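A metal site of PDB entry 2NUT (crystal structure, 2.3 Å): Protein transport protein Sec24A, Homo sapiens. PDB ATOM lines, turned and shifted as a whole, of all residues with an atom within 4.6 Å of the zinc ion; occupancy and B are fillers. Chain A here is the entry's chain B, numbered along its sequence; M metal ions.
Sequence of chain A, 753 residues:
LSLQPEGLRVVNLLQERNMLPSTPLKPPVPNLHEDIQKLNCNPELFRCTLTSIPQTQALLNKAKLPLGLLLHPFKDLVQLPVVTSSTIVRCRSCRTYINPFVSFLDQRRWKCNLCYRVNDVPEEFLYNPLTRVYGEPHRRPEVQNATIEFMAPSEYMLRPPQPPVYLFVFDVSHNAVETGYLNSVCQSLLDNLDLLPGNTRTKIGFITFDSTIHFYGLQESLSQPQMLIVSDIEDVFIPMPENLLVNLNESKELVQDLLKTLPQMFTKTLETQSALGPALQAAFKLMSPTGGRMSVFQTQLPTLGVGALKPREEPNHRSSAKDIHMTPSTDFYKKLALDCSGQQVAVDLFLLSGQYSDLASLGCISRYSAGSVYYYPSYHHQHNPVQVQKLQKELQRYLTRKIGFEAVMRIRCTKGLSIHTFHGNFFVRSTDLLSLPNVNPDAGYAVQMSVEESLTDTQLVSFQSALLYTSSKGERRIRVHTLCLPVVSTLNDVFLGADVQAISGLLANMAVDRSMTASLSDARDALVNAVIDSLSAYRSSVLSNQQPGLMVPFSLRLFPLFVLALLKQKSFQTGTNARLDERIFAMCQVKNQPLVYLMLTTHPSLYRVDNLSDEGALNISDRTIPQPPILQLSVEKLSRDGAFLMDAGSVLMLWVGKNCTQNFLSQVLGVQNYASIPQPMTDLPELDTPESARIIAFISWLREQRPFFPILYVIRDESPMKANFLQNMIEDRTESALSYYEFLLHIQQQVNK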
ATOM      1  N   CYS A  91       1.181  26.097 -27.202  1.00  0.00           N
ATOM      2  CA  CYS A  91       0.019  25.500 -26.577  1.00  0.00           C
ATOM      3  C   CYS A  91      -0.725  24.646 -27.585  1.00  0.00           C
ATOM      4  O   CYS A  91      -0.977  25.081 -28.710  1.00  0.00           O
ATOM      5  CB  CYS A  91      -0.920  26.572 -26.031  1.00  0.00           C
ATOM      6  SG  CYS A  91      -2.481  25.887 -25.463  1.00  0.00           S
ATOM      7  N   SER A  93      -3.699  23.970 -27.762  1.00  0.00           N
ATOM      8  CA  SER A  93      -5.022  24.482 -28.089  1.00  0.00           C
ATOM      9  C   SER A  93      -5.026  25.714 -28.961  1.00  0.00           C
ATOM     10  O   SER A  93      -5.448  25.657 -30.109  1.00  0.00           O
ATOM     11  CB  SER A  93      -5.801  24.782 -26.802  1.00  0.00           C
ATOM     12  OG  SER A  93      -6.100  23.601 -26.090  1.00  0.00           O
ATOM     13  N   CYS A  94      -4.544  26.836 -28.412  1.00  0.00           N
ATOM     14  CA  CYS A  94      -4.527  28.105 -29.137  1.00  0.00           C
ATOM     15  C   CYS A  94      -3.217  28.457 -29.848  1.00  0.00           C
ATOM     16  O   CYS A  94      -3.053  29.566 -30.319  1.00  0.00           O
ATOM     17  CB  CYS A  94      -4.877  29.253 -28.173  1.00  0.00           C
ATOM     18  SG  CYS A  94      -3.545  29.651 -27.013  1.00  0.00           S
ATOM     19  N   THR A  96      -0.424  29.272 -28.803  1.00  0.00           N
ATOM     20  CA  THR A  96       0.360  30.333 -28.176  1.00  0.00           C
ATOM     21  C   THR A  96       1.773  29.861 -27.813  1.00  0.00           C
ATOM     22  O   THR A  96       1.964  28.731 -27.344  1.00  0.00           O
ATOM     23  CB  THR A  96      -0.348  30.868 -26.904  1.00  0.00           C
ATOM     24  OG1 THR A  96      -1.489  31.656 -27.292  1.00  0.00           O
ATOM     25  CG2 THR A  96       0.600  31.708 -26.074  1.00  0.00           C
ATOM     26  N   CYS A 112      -1.305  27.413 -19.977  1.00  0.00           N
ATOM     27  CA  CYS A 112      -1.297  28.524 -20.937  1.00  0.00           C
ATOM     28  C   CYS A 112      -1.914  29.796 -20.367  1.00  0.00           C
ATOM     29  O   CYS A 112      -3.056  29.802 -19.913  1.00  0.00           O
ATOM     30  CB  CYS A 112      -2.062  28.116 -22.212  1.00  0.00           C
ATOM     31  SG  CYS A 112      -2.231  29.414 -23.510  1.00  0.00           S
ATOM     32  N   CYS A 115      -5.250  30.588 -22.858  1.00  0.00           N
ATOM     33  CA  CYS A 115      -6.483  29.806 -22.997  1.00  0.00           C
ATOM     34  C   CYS A 115      -6.677  28.888 -21.807  1.00  0.00           C
ATOM     35  O   CYS A 115      -7.675  28.159 -21.726  1.00  0.00           O
ATOM     36  CB  CYS A 115      -6.468  28.989 -24.292  1.00  0.00           C
ATOM     37  SG  CYS A 115      -5.633  27.424 -24.139  1.00  0.00           S
HETATM   38 ZN    ZN M   1      -3.488  28.103 -25.064  1.00  0.00          ZN
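The side-chain sulfur (SG) of Cys 91 sits close to the backbone NH (N) of Ser 93, 3.2 Å away.
N of Cys 91 sits at hydrogen-bond distance from O of Thr 96, at 2.8 Å.
The side-chain hydroxyl of Thr 96 sits close to the side-chain sulfur of Cys 94 (2.9 Å).
The zinc ion is bound by the side-chain sulfur of Cys 112 (2.4 Å), the side-chain sulfur of Cys 115 (2.4 Å), the side-chain sulfur of Cys 91 (2.5 Å) and the side-chain sulfur of Cys 94 (2.5 Å).
The zinc ion has four donor atoms within binding distance.
The nearest printed residue that does not touch the zinc ion is Ser 93 (4.4 Å).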
